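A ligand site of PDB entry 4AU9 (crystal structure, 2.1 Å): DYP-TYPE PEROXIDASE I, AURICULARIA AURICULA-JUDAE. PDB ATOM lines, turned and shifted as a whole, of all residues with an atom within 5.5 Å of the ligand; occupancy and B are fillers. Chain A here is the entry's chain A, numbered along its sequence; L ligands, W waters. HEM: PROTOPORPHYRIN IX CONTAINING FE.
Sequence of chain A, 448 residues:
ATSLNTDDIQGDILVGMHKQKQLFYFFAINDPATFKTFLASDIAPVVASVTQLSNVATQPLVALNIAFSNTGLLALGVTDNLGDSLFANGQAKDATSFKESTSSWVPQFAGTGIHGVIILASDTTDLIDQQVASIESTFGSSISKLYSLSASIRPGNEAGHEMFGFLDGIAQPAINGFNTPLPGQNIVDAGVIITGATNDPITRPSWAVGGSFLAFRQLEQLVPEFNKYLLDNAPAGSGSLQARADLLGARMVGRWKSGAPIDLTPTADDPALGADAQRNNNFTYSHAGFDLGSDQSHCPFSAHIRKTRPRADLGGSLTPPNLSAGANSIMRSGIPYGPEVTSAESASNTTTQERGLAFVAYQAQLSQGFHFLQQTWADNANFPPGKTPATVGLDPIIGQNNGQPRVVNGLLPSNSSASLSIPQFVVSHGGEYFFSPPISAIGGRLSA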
ATOM      1  N   GLU A 162      -9.971  31.564   5.022  1.00  0.00           N
ATOM      2  CA  GLU A 162      -8.568  31.956   4.819  1.00  0.00           C
ATOM      3  C   GLU A 162      -8.449  33.343   4.168  1.00  0.00           C
ATOM      4  O   GLU A 162      -9.471  33.984   3.851  1.00  0.00           O
ATOM      5  CB  GLU A 162      -7.818  30.890   4.016  1.00  0.00           C
ATOM      6  CG  GLU A 162      -8.526  30.416   2.730  1.00  0.00           C
ATOM      7  CD  GLU A 162      -8.466  31.455   1.632  1.00  0.00           C
ATOM      8  OE1 GLU A 162      -7.340  31.890   1.321  1.00  0.00           O
ATOM      9  OE2 GLU A 162      -9.532  31.913   1.160  1.00  0.00           O
ATOM     10  N   PHE A 164      -7.604  34.680   1.323  1.00  0.00           N
ATOM     11  CA  PHE A 164      -8.231  34.972   0.012  1.00  0.00           C
ATOM     12  C   PHE A 164      -9.759  35.107   0.126  1.00  0.00           C
ATOM     13  O   PHE A 164     -10.436  35.475  -0.837  1.00  0.00           O
ATOM     14  CB  PHE A 164      -7.895  33.907  -1.022  1.00  0.00           C
ATOM     15  CG  PHE A 164      -6.459  33.916  -1.493  1.00  0.00           C
ATOM     16  CD1 PHE A 164      -5.762  35.106  -1.702  1.00  0.00           C
ATOM     17  CD2 PHE A 164      -5.820  32.720  -1.807  1.00  0.00           C
ATOM     18  CE1 PHE A 164      -4.453  35.098  -2.200  1.00  0.00           C
ATOM     19  CE2 PHE A 164      -4.494  32.699  -2.268  1.00  0.00           C
ATOM     20  CZ  PHE A 164      -3.835  33.892  -2.491  1.00  0.00           C
ATOM     21  N   PHE A 166     -11.859  32.403   1.295  1.00  0.00           N
ATOM     22  CA  PHE A 166     -12.534  31.090   1.048  1.00  0.00           C
ATOM     23  C   PHE A 166     -12.649  30.304   2.338  1.00  0.00           C
ATOM     24  O   PHE A 166     -11.643  30.129   3.049  1.00  0.00           O
ATOM     25  CB  PHE A 166     -11.802  30.253  -0.016  1.00  0.00           C
ATOM     26  CG  PHE A 166     -11.916  30.828  -1.425  1.00  0.00           C
ATOM     27  CD1 PHE A 166     -11.100  31.888  -1.825  1.00  0.00           C
ATOM     28  CD2 PHE A 166     -12.953  30.442  -2.271  1.00  0.00           C
ATOM     29  CE1 PHE A 166     -11.269  32.513  -3.084  1.00  0.00           C
ATOM     30  CE2 PHE A 166     -13.105  31.002  -3.527  1.00  0.00           C
ATOM     31  CZ  PHE A 166     -12.269  32.088  -3.926  1.00  0.00           C
ATOM     32  N   LEU A 167     -13.870  29.886   2.662  1.00  0.00           N
ATOM     33  CA  LEU A 167     -14.104  28.959   3.778  1.00  0.00           C
ATOM     34  C   LEU A 167     -13.180  27.820   3.592  1.00  0.00           C
ATOM     35  O   LEU A 167     -13.086  27.267   2.493  1.00  0.00           O
ATOM     36  CB  LEU A 167     -15.523  28.379   3.789  1.00  0.00           C
ATOM     37  CG  LEU A 167     -15.933  27.659   5.089  1.00  0.00           C
ATOM     38  CD1 LEU A 167     -15.917  28.585   6.298  1.00  0.00           C
ATOM     39  CD2 LEU A 167     -17.322  27.011   4.953  1.00  0.00           C
ATOM     40  N   ASP A 168     -12.407  27.547   4.630  1.00  0.00           N
ATOM     41  CA  ASP A 168     -11.527  26.401   4.599  1.00  0.00           C
ATOM     42  C   ASP A 168     -11.909  25.386   5.665  1.00  0.00           C
ATOM     43  O   ASP A 168     -12.981  25.497   6.279  1.00  0.00           O
ATOM     44  CB  ASP A 168     -10.059  26.803   4.688  1.00  0.00           C
ATOM     45  CG  ASP A 168      -9.132  25.600   4.623  1.00  0.00           C
ATOM     46  OD1 ASP A 168      -9.571  24.534   5.083  1.00  0.00           O
ATOM     47  OD2 ASP A 168      -8.010  25.716   4.082  1.00  0.00           O
ATOM     48  N   GLY A 169     -11.142  24.309   5.756  1.00  0.00           N
ATOM     49  CA  GLY A 169     -11.467  23.216   6.683  1.00  0.00           C
ATOM     50  C   GLY A 169     -12.823  22.540   6.509  1.00  0.00           C
ATOM     51  O   GLY A 169     -13.409  22.082   7.492  1.00  0.00           O
ATOM     52  N   ILE A 170     -13.329  22.454   5.288  1.00  0.00           N
ATOM     53  CA  ILE A 170     -14.477  21.588   5.024  1.00  0.00           C
ATOM     54  C   ILE A 170     -14.066  20.102   4.937  1.00  0.00           C
ATOM     55  O   ILE A 170     -14.783  19.229   5.409  1.00  0.00           O
ATOM     56  CB  ILE A 170     -15.202  21.931   3.694  1.00  0.00           C
ATOM     57  CG1 ILE A 170     -15.932  23.267   3.817  1.00  0.00           C
ATOM     58  CG2 ILE A 170     -16.286  20.845   3.424  1.00  0.00           C
ATOM     59  CD1 ILE A 170     -15.837  24.145   2.592  1.00  0.00           C
ATOM     60  N   ALA A 171     -12.924  19.840   4.312  1.00  0.00           N
ATOM     61  CA  ALA A 171     -12.582  18.522   3.812  1.00  0.00           C
ATOM     62  C   ALA A 171     -11.392  17.917   4.559  1.00  0.00           C
ATOM     63  O   ALA A 171     -10.313  18.522   4.625  1.00  0.00           O
ATOM     64  CB  ALA A 171     -12.298  18.587   2.301  1.00  0.00           C
ATOM     65  N   GLN A 172     -11.607  16.734   5.121  1.00  0.00           N
ATOM     66  CA  GLN A 172     -10.554  15.991   5.804  1.00  0.00           C
ATOM     67  C   GLN A 172     -10.846  14.505   5.594  1.00  0.00           C
ATOM     68  O   GLN A 172     -12.000  14.123   5.429  1.00  0.00           O
ATOM     69  CB  GLN A 172     -10.533  16.307   7.317  1.00  0.00           C
ATOM     70  CG  GLN A 172     -10.555  17.784   7.681  1.00  0.00           C
ATOM     71  CD  GLN A 172      -9.147  18.426   7.730  1.00  0.00           C
ATOM     72  OE1 GLN A 172      -8.152  17.833   7.281  1.00  0.00           O
ATOM     73  NE2 GLN A 172      -9.087  19.666   8.212  1.00  0.00           N
ATOM     74  N   LEU A 219       3.134  30.353   4.572  1.00  0.00           N
ATOM     75  CA  LEU A 219       2.839  30.612   3.154  1.00  0.00           C
ATOM     76  C   LEU A 219       2.227  32.005   3.018  1.00  0.00           C
ATOM     77  O   LEU A 219       1.065  32.203   3.375  1.00  0.00           O
ATOM     78  CB  LEU A 219       1.846  29.570   2.605  1.00  0.00           C
ATOM     79  CG  LEU A 219       2.312  28.091   2.613  1.00  0.00           C
ATOM     80  CD1 LEU A 219       1.233  27.143   2.171  1.00  0.00           C
ATOM     81  CD2 LEU A 219       3.596  27.837   1.774  1.00  0.00           C
ATOM     82  N   GLN A 221       0.389  35.038   1.407  1.00  0.00           N
ATOM     83  CA  GLN A 221      -0.642  35.183   0.396  1.00  0.00           C
ATOM     84  C   GLN A 221      -0.735  36.639  -0.074  1.00  0.00           C
ATOM     85  O   GLN A 221      -0.844  37.532   0.740  1.00  0.00           O
ATOM     86  CB  GLN A 221      -1.980  34.796   1.023  1.00  0.00           C
ATOM     87  CG  GLN A 221      -2.225  33.287   1.091  1.00  0.00           C
ATOM     88  CD  GLN A 221      -3.501  32.943   1.832  1.00  0.00           C
ATOM     89  OE1 GLN A 221      -3.487  32.686   3.031  1.00  0.00           O
ATOM     90  NE2 GLN A 221      -4.630  32.931   1.117  1.00  0.00           N
ATOM     91  N   VAL A 253     -10.123  27.731  -7.110  1.00  0.00           N
ATOM     92  CA  VAL A 253     -10.143  27.013  -5.823  1.00  0.00           C
ATOM     93  C   VAL A 253     -10.826  25.650  -5.976  1.00  0.00           C
ATOM     94  O   VAL A 253     -10.317  24.629  -5.503  1.00  0.00           O
ATOM     95  CB  VAL A 253     -10.865  27.852  -4.708  1.00  0.00           C
ATOM     96  CG1 VAL A 253     -10.976  27.044  -3.420  1.00  0.00           C
ATOM     97  CG2 VAL A 253     -10.069  29.148  -4.420  1.00  0.00           C
ATOM     98  N   ARG A 255     -14.141  25.764  -5.118  1.00  0.00           N
ATOM     99  CA  ARG A 255     -15.302  26.037  -4.228  1.00  0.00           C
ATOM    100  C   ARG A 255     -15.500  27.523  -4.257  1.00  0.00           C
ATOM    101  O   ARG A 255     -14.522  28.265  -4.321  1.00  0.00           O
ATOM    102  CB  ARG A 255     -15.008  25.682  -2.754  1.00  0.00           C
ATOM    103  CG  ARG A 255     -14.769  24.193  -2.478  1.00  0.00           C
ATOM    104  CD  ARG A 255     -14.747  23.876  -0.971  1.00  0.00           C
ATOM    105  NE  ARG A 255     -14.547  22.460  -0.732  1.00  0.00           N
ATOM    106  CZ  ARG A 255     -15.537  21.596  -0.561  1.00  0.00           C
ATOM    107  NH1 ARG A 255     -16.790  22.041  -0.518  1.00  0.00           N
ATOM    108  NH2 ARG A 255     -15.274  20.300  -0.354  1.00  0.00           N
ATOM    109  N   ASN A 281     -19.603  18.200   0.554  1.00  0.00           N
ATOM    110  CA  ASN A 281     -18.508  17.341   0.092  1.00  0.00           C
ATOM    111  C   ASN A 281     -18.981  16.152  -0.700  1.00  0.00           C
ATOM    112  O   ASN A 281     -18.214  15.242  -1.023  1.00  0.00           O
ATOM    113  CB  ASN A 281     -17.614  16.848   1.240  1.00  0.00           C
ATOM    114  CG  ASN A 281     -16.125  16.850   0.866  1.00  0.00           C
ATOM    115  OD1 ASN A 281     -15.728  17.469  -0.126  1.00  0.00           O
ATOM    116  ND2 ASN A 281     -15.309  16.092   1.620  1.00  0.00           N
ATOM    117  N   TYR A 285     -16.623  14.488  -8.826  1.00  0.00           N
ATOM    118  CA  TYR A 285     -16.302  15.016 -10.159  1.00  0.00           C
ATOM    119  C   TYR A 285     -17.018  14.397 -11.372  1.00  0.00           C
ATOM    120  O   TYR A 285     -17.123  15.029 -12.407  1.00  0.00           O
ATOM    121  CB  TYR A 285     -14.791  15.188 -10.390  1.00  0.00           C
ATOM    122  CG  TYR A 285     -14.135  16.054  -9.316  1.00  0.00           C
ATOM    123  CD1 TYR A 285     -14.527  17.374  -9.114  1.00  0.00           C
ATOM    124  CD2 TYR A 285     -13.199  15.511  -8.456  1.00  0.00           C
ATOM    125  CE1 TYR A 285     -13.930  18.163  -8.123  1.00  0.00           C
ATOM    126  CE2 TYR A 285     -12.587  16.270  -7.460  1.00  0.00           C
ATOM    127  CZ  TYR A 285     -12.985  17.576  -7.266  1.00  0.00           C
ATOM    128  OH  TYR A 285     -12.400  18.283  -6.246  1.00  0.00           O
ATOM    129  N   HIS A 304      -7.486  23.838  -7.409  1.00  0.00           N
ATOM    130  CA  HIS A 304      -6.794  23.414  -6.173  1.00  0.00           C
ATOM    131  C   HIS A 304      -7.283  22.116  -5.509  1.00  0.00           C
ATOM    132  O   HIS A 304      -6.475  21.235  -5.273  1.00  0.00           O
ATOM    133  CB  HIS A 304      -6.644  24.582  -5.211  1.00  0.00           C
ATOM    134  CG  HIS A 304      -6.107  24.224  -3.856  1.00  0.00           C
ATOM    135  ND1 HIS A 304      -4.809  23.840  -3.643  1.00  0.00           N
ATOM    136  CD2 HIS A 304      -6.659  24.341  -2.617  1.00  0.00           C
ATOM    137  CE1 HIS A 304      -4.585  23.696  -2.336  1.00  0.00           C
ATOM    138  NE2 HIS A 304      -5.711  23.964  -1.697  1.00  0.00           N
ATOM    139  N   ILE A 305      -8.542  22.029  -5.079  1.00  0.00           N
ATOM    140  CA  ILE A 305      -9.001  20.847  -4.319  1.00  0.00           C
ATOM    141  C   ILE A 305      -9.064  19.592  -5.178  1.00  0.00           C
ATOM    142  O   ILE A 305      -8.927  18.475  -4.677  1.00  0.00           O
ATOM    143  CB  ILE A 305     -10.401  21.053  -3.656  1.00  0.00           C
ATOM    144  CG1 ILE A 305     -11.495  21.330  -4.703  1.00  0.00           C
ATOM    145  CG2 ILE A 305     -10.357  22.148  -2.663  1.00  0.00           C
ATOM    146  CD1 ILE A 305     -12.973  21.096  -4.143  1.00  0.00           C
ATOM    147  N   THR A 308      -5.442  18.398  -5.329  1.00  0.00           N
ATOM    148  CA  THR A 308      -4.972  17.827  -4.084  1.00  0.00           C
ATOM    149  C   THR A 308      -5.816  16.650  -3.546  1.00  0.00           C
ATOM    150  O   THR A 308      -5.296  15.851  -2.803  1.00  0.00           O
ATOM    151  CB  THR A 308      -4.830  18.882  -2.994  1.00  0.00           C
ATOM    152  OG1 THR A 308      -6.124  19.443  -2.743  1.00  0.00           O
ATOM    153  CG2 THR A 308      -3.862  19.976  -3.401  1.00  0.00           C
ATOM    154  N   ARG A 309      -7.104  16.570  -3.872  1.00  0.00           N
ATOM    155  CA  ARG A 309      -7.829  15.290  -3.793  1.00  0.00           C
ATOM    156  C   ARG A 309      -8.603  14.944  -5.070  1.00  0.00           C
ATOM    157  O   ARG A 309      -9.717  15.408  -5.285  1.00  0.00           O
ATOM    158  CB  ARG A 309      -8.723  15.158  -2.539  1.00  0.00           C
ATOM    159  CG  ARG A 309      -9.445  13.759  -2.405  1.00  0.00           C
ATOM    160  CD  ARG A 309     -10.728  13.815  -1.542  1.00  0.00           C
ATOM    161  NE  ARG A 309     -11.468  12.550  -1.579  1.00  0.00           N
ATOM    162  CZ  ARG A 309     -12.705  12.370  -1.126  1.00  0.00           C
ATOM    163  NH1 ARG A 309     -13.378  13.364  -0.549  1.00  0.00           N
ATOM    164  NH2 ARG A 309     -13.299  11.189  -1.291  1.00  0.00           N
ATOM    165  N   ARG A 311     -10.212  12.492  -6.317  1.00  0.00           N
ATOM    166  CA  ARG A 311     -11.450  11.698  -6.348  1.00  0.00           C
ATOM    167  C   ARG A 311     -11.553  10.829  -7.603  1.00  0.00           C
ATOM    168  O   ARG A 311     -10.625  10.079  -7.951  1.00  0.00           O
ATOM    169  CB  ARG A 311     -12.677  12.618  -6.189  1.00  0.00           C
ATOM    170  CG  ARG A 311     -12.553  13.580  -5.011  1.00  0.00           C
ATOM    171  CD  ARG A 311     -13.862  14.244  -4.609  1.00  0.00           C
ATOM    172  NE  ARG A 311     -13.628  15.284  -3.620  1.00  0.00           N
ATOM    173  CZ  ARG A 311     -14.499  15.692  -2.706  1.00  0.00           C
ATOM    174  NH1 ARG A 311     -15.668  15.066  -2.561  1.00  0.00           N
ATOM    175  NH2 ARG A 311     -14.146  16.655  -1.842  1.00  0.00           N
ATOM    176  N   ILE A 330      -3.832  13.974   3.772  1.00  0.00           N
ATOM    177  CA  ILE A 330      -3.262  14.729   4.877  1.00  0.00           C
ATOM    178  C   ILE A 330      -4.424  15.244   5.766  1.00  0.00           C
ATOM    179  O   ILE A 330      -5.474  15.605   5.241  1.00  0.00           O
ATOM    180  CB  ILE A 330      -2.384  15.925   4.356  1.00  0.00           C
ATOM    181  CG1 ILE A 330      -3.199  16.851   3.444  1.00  0.00           C
ATOM    182  CG2 ILE A 330      -1.182  15.391   3.571  1.00  0.00           C
ATOM    183  CD1 ILE A 330      -2.551  18.199   3.158  1.00  0.00           C
ATOM    184  N   ARG A 332      -5.423  18.456   7.862  1.00  0.00           N
ATOM    185  CA  ARG A 332      -5.039  19.871   7.761  1.00  0.00           C
ATOM    186  C   ARG A 332      -5.399  20.659   8.999  1.00  0.00           C
ATOM    187  O   ARG A 332      -6.524  20.651   9.440  1.00  0.00           O
ATOM    188  CB  ARG A 332      -5.676  20.532   6.541  1.00  0.00           C
ATOM    189  CG  ARG A 332      -4.963  20.155   5.281  1.00  0.00           C
ATOM    190  CD  ARG A 332      -5.725  20.550   4.024  1.00  0.00           C
ATOM    191  NE  ARG A 332      -7.165  20.331   4.087  1.00  0.00           N
ATOM    192  CZ  ARG A 332      -8.083  21.301   3.960  1.00  0.00           C
ATOM    193  NH1 ARG A 332      -7.725  22.580   3.939  1.00  0.00           N
ATOM    194  NH2 ARG A 332      -9.375  20.982   4.029  1.00  0.00           N
ATOM    195  N   LEU A 357      -1.120  32.043   5.385  1.00  0.00           N
ATOM    196  CA  LEU A 357      -1.571  30.836   6.086  1.00  0.00           C
ATOM    197  C   LEU A 357      -0.368  30.176   6.760  1.00  0.00           C
ATOM    198  O   LEU A 357       0.678  29.960   6.138  1.00  0.00           O
ATOM    199  CB  LEU A 357      -2.208  29.846   5.116  1.00  0.00           C
ATOM    200  CG  LEU A 357      -2.741  28.493   5.624  1.00  0.00           C
ATOM    201  CD1 LEU A 357      -4.087  28.627   6.384  1.00  0.00           C
ATOM    202  CD2 LEU A 357      -2.918  27.523   4.473  1.00  0.00           C
ATOM    203  N   PHE A 359       0.582  26.909   7.462  1.00  0.00           N
ATOM    204  CA  PHE A 359      -0.011  25.745   6.873  1.00  0.00           C
ATOM    205  C   PHE A 359       0.569  24.593   7.658  1.00  0.00           C
ATOM    206  O   PHE A 359       1.779  24.571   7.933  1.00  0.00           O
ATOM    207  CB  PHE A 359       0.296  25.645   5.375  1.00  0.00           C
ATOM    208  CG  PHE A 359      -0.082  24.294   4.772  1.00  0.00           C
ATOM    209  CD1 PHE A 359       0.821  23.249   4.795  1.00  0.00           C
ATOM    210  CD2 PHE A 359      -1.344  24.072   4.246  1.00  0.00           C
ATOM    211  CE1 PHE A 359       0.466  21.987   4.280  1.00  0.00           C
ATOM    212  CE2 PHE A 359      -1.720  22.795   3.808  1.00  0.00           C
ATOM    213  CZ  PHE A 359      -0.784  21.772   3.793  1.00  0.00           C
ATOM    214  N   PHE A 370       2.069  15.616   2.329  1.00  0.00           N
ATOM    215  CA  PHE A 370       2.327  17.000   1.866  1.00  0.00           C
ATOM    216  C   PHE A 370       3.254  17.030   0.642  1.00  0.00           C
ATOM    217  O   PHE A 370       2.948  17.628  -0.371  1.00  0.00           O
ATOM    218  CB  PHE A 370       2.962  17.849   2.983  1.00  0.00           C
ATOM    219  CG  PHE A 370       3.655  19.086   2.476  1.00  0.00           C
ATOM    220  CD1 PHE A 370       2.911  20.159   1.995  1.00  0.00           C
ATOM    221  CD2 PHE A 370       5.037  19.153   2.398  1.00  0.00           C
ATOM    222  CE1 PHE A 370       3.536  21.255   1.388  1.00  0.00           C
ATOM    223  CE2 PHE A 370       5.691  20.257   1.866  1.00  0.00           C
ATOM    224  CZ  PHE A 370       4.939  21.330   1.367  1.00  0.00           C
ATOM    225  N   LEU A 373       1.584  15.464  -2.556  1.00  0.00           N
ATOM    226  CA  LEU A 373       0.575  16.367  -3.127  1.00  0.00           C
ATOM    227  C   LEU A 373       1.210  17.569  -3.840  1.00  0.00           C
ATOM    228  O   LEU A 373       0.727  18.062  -4.878  1.00  0.00           O
ATOM    229  CB  LEU A 373      -0.373  16.886  -2.032  1.00  0.00           C
ATOM    230  CG  LEU A 373      -1.631  16.084  -1.663  1.00  0.00           C
ATOM    231  CD1 LEU A 373      -1.457  14.550  -1.767  1.00  0.00           C
ATOM    232  CD2 LEU A 373      -2.122  16.474  -0.278  1.00  0.00           C
ATOM    233  N   GLN A 374       2.286  18.077  -3.270  1.00  0.00           N
ATOM    234  CA  GLN A 374       2.803  19.341  -3.737  1.00  0.00           C
ATOM    235  C   GLN A 374       3.549  19.127  -5.070  1.00  0.00           C
ATOM    236  O   GLN A 374       3.323  19.854  -6.036  1.00  0.00           O
ATOM    237  CB  GLN A 374       3.717  19.966  -2.688  1.00  0.00           C
ATOM    238  CG  GLN A 374       4.471  21.202  -3.215  1.00  0.00           C
ATOM    239  CD  GLN A 374       3.596  22.445  -3.232  1.00  0.00           C
ATOM    240  OE1 GLN A 374       3.087  22.851  -2.195  1.00  0.00           O
ATOM    241  NE2 GLN A 374       3.282  22.926  -4.408  1.00  0.00           N
ATOM    242  N   ILE A 397      -3.203  27.880  -7.121  1.00  0.00           N
ATOM    243  CA  ILE A 397      -3.020  28.349  -5.757  1.00  0.00           C
ATOM    244  C   ILE A 397      -1.631  27.995  -5.254  1.00  0.00           C
ATOM    245  O   ILE A 397      -0.910  28.880  -4.814  1.00  0.00           O
ATOM    246  CB  ILE A 397      -4.088  27.776  -4.803  1.00  0.00           C
ATOM    247  CG1 ILE A 397      -5.502  28.090  -5.315  1.00  0.00           C
ATOM    248  CG2 ILE A 397      -3.868  28.280  -3.390  1.00  0.00           C
ATOM    249  CD1 ILE A 397      -5.883  29.583  -5.299  1.00  0.00           C
ATOM    250  N   ILE A 398      -1.246  26.712  -5.319  1.00  0.00           N
ATOM    251  CA  ILE A 398       0.026  26.324  -4.737  1.00  0.00           C
ATOM    252  C   ILE A 398       1.069  25.851  -5.734  1.00  0.00           C
ATOM    253  O   ILE A 398       2.170  25.506  -5.335  1.00  0.00           O
ATOM    254  CB  ILE A 398      -0.133  25.259  -3.657  1.00  0.00           C
ATOM    255  CG1 ILE A 398      -0.897  24.025  -4.172  1.00  0.00           C
ATOM    256  CG2 ILE A 398      -0.779  25.848  -2.432  1.00  0.00           C
ATOM    257  CD1 ILE A 398      -0.695  22.826  -3.290  1.00  0.00           C
ATOM    258  N   VAL A 426       0.962  33.050  -3.913  1.00  0.00           N
ATOM    259  CA  VAL A 426       1.303  32.443  -2.649  1.00  0.00           C
ATOM    260  C   VAL A 426       2.782  32.202  -2.704  1.00  0.00           C
ATOM    261  O   VAL A 426       3.272  31.707  -3.708  1.00  0.00           O
ATOM    262  CB  VAL A 426       0.565  31.112  -2.485  1.00  0.00           C
ATOM    263  CG1 VAL A 426       1.118  30.368  -1.235  1.00  0.00           C
ATOM    264  CG2 VAL A 426      -0.922  31.410  -2.315  1.00  0.00           C
HETATM  265  CHA HEM L   1      -8.552  22.479   0.481  1.00  0.00           C
HETATM  266  CHB HEM L   1      -6.872  27.044   0.525  1.00  0.00           C
HETATM  267  CHC HEM L   1      -2.337  25.363   0.688  1.00  0.00           C
HETATM  268  CHD HEM L   1      -3.922  20.798   0.352  1.00  0.00           C
HETATM  269  C1A HEM L   1      -8.500  23.854   0.475  1.00  0.00           C
HETATM  270  C2A HEM L   1      -9.646  24.764   0.382  1.00  0.00           C
HETATM  271  C3A HEM L   1      -9.181  26.016   0.443  1.00  0.00           C
HETATM  272  C4A HEM L   1      -7.718  25.950   0.550  1.00  0.00           C
HETATM  273  CMA HEM L   1     -10.014  27.316   0.383  1.00  0.00           C
HETATM  274  CAA HEM L   1     -11.148  24.356   0.388  1.00  0.00           C
HETATM  275  CBA HEM L   1     -11.544  24.043   1.834  1.00  0.00           C
HETATM  276  CGA HEM L   1     -11.835  22.574   2.024  1.00  0.00           C
HETATM  277  O1A HEM L   1     -12.086  21.863   1.007  1.00  0.00           O
HETATM  278  O2A HEM L   1     -11.836  22.111   3.199  1.00  0.00           O
HETATM  279  C1B HEM L   1      -5.491  27.005   0.572  1.00  0.00           C
HETATM  280  C2B HEM L   1      -4.582  28.142   0.549  1.00  0.00           C
HETATM  281  C3B HEM L   1      -3.310  27.683   0.664  1.00  0.00           C
HETATM  282  C4B HEM L   1      -3.390  26.231   0.651  1.00  0.00           C
HETATM  283  CMB HEM L   1      -5.092  29.600   0.474  1.00  0.00           C
HETATM  284  CAB HEM L   1      -1.974  28.467   0.591  1.00  0.00           C
HETATM  285  CBB HEM L   1      -1.791  29.687   1.169  1.00  0.00           C
HETATM  286  C1C HEM L   1      -2.365  23.970   0.570  1.00  0.00           C
HETATM  287  C2C HEM L   1      -1.197  23.087   0.440  1.00  0.00           C
HETATM  288  C3C HEM L   1      -1.637  21.818   0.257  1.00  0.00           C
HETATM  289  C4C HEM L   1      -3.077  21.868   0.395  1.00  0.00           C
HETATM  290  CMC HEM L   1       0.275  23.562   0.437  1.00  0.00           C
HETATM  291  CAC HEM L   1      -0.812  20.519   0.187  1.00  0.00           C
HETATM  292  CBC HEM L   1       0.247  20.353  -0.632  1.00  0.00           C
HETATM  293  C1D HEM L   1      -5.306  20.843   0.507  1.00  0.00           C
HETATM  294  C2D HEM L   1      -6.154  19.672   0.534  1.00  0.00           C
HETATM  295  C3D HEM L   1      -7.586  20.174   0.519  1.00  0.00           C
HETATM  296  C4D HEM L   1      -7.479  21.603   0.430  1.00  0.00           C
HETATM  297  CMD HEM L   1      -5.725  18.200   0.594  1.00  0.00           C
HETATM  298  CAD HEM L   1      -8.852  19.314   0.625  1.00  0.00           C
HETATM  299  CBD HEM L   1      -9.271  18.895  -0.781  1.00  0.00           C
HETATM  300  CGD HEM L   1     -10.344  17.851  -0.667  1.00  0.00           C
HETATM  301  O1D HEM L   1     -11.182  17.761  -1.592  1.00  0.00           O
HETATM  302  O2D HEM L   1     -10.312  17.053   0.327  1.00  0.00           O
HETATM  303  NA  HEM L   1      -7.350  24.605   0.483  1.00  0.00           N
HETATM  304  NB  HEM L   1      -4.727  25.877   0.542  1.00  0.00           N
HETATM  305  NC  HEM L   1      -3.476  23.190   0.389  1.00  0.00           N
HETATM  306  ND  HEM L   1      -6.125  21.944   0.353  1.00  0.00           N
HETATM  307 FE   HEM L   1      -5.425  23.896   0.380  1.00  0.00          FE
HETATM  308  O   HOH W   1     -12.625  15.547   0.932  1.00  0.00           O
HETATM  309  O   HOH W   2     -11.497  17.201  -4.206  1.00  0.00           O
HETATM  310  O   HOH W   3     -12.445  20.064  -0.860  1.00  0.00           O
HETATM  311  O   HOH W   4      -8.730  15.974   2.135  1.00  0.00           O
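An iron atom (FE) of the ligand is bound by a ring nitrogen (NE2) of His 304, 2.1 Å away. N of Ile 170 is in hydrogen-bond range of O2A of the ligand (2.6 Å). The backbone NH of Ala 171 sits at hydrogen-bond distance from an oxygen (O2A) of the ligand (2.8 Å). The guanidinium group (NH2) of Arg 332 is in salt-bridge range of an oxygen (O2A) of the ligand (2.8 Å). NE of Arg 255 lies within salt-bridge range of O1A of the ligand, 3.1 Å away. NH2 of Arg 311 lies within salt-bridge range of O1D of the ligand (3.2 Å). The backbone NH of Gly 169 lies within hydrogen-bond range of an oxygen (O2A) of the ligand.
O of Ala 171 sits at hydrogen-bond distance from NH2 of Arg 332 (2.7 Å). NH2 of Arg 255 sits at hydrogen-bond distance from OD1 of Asn 281, 2.9 Å away. The guanidinium group (NH2) of Arg 311 sits at hydrogen-bond distance from the side-chain amide oxygen (OD1) of Asn 281 (2.5 Å). The backbone NH (N) of Leu 357 is in hydrogen-bond range of the side-chain amide oxygen (OE1) of Gln 221, 3.4 Å away. The side-chain amide nitrogen of Gln 221 sits close to the backbone NH of Phe 164. The backbone carbonyl oxygen (O) of Ile 398 lies within hydrogen-bond range of the side-chain amide nitrogen (NE2) of Gln 374, 3.0 Å away. The backbone NH (N) of Ile 305 sits at hydrogen-bond distance from the backbone carbonyl oxygen (O) of Val 253, at 3.2 Å. N of Leu 219 lies within hydrogen-bond range of O of Leu 357 (2.9 Å).
Merely in contact with the ligand: Thr 308, Glu 162, Phe 359, Gln 221, Phe 166, Ile 398, Asp 168, Leu 167, Ile 305, Arg 309, Phe 370, Leu 373, Leu 219, Leu 357, Val 426, Gln 374, Val 253 and Phe 164.
Water W3 bridges an oxygen (O1A) of the ligand (2.6 Å) and the guanidinium group (NH2) of Arg 255 (2.9 Å). Water W2 lies within hydrogen-bond range of OH of Tyr 285 (2.5 Å), O1D of the ligand (2.7 Å), O of Arg 309 (2.7 Å), O of Ile 305 (2.9 Å) and NE of Arg 311 (2.9 Å).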
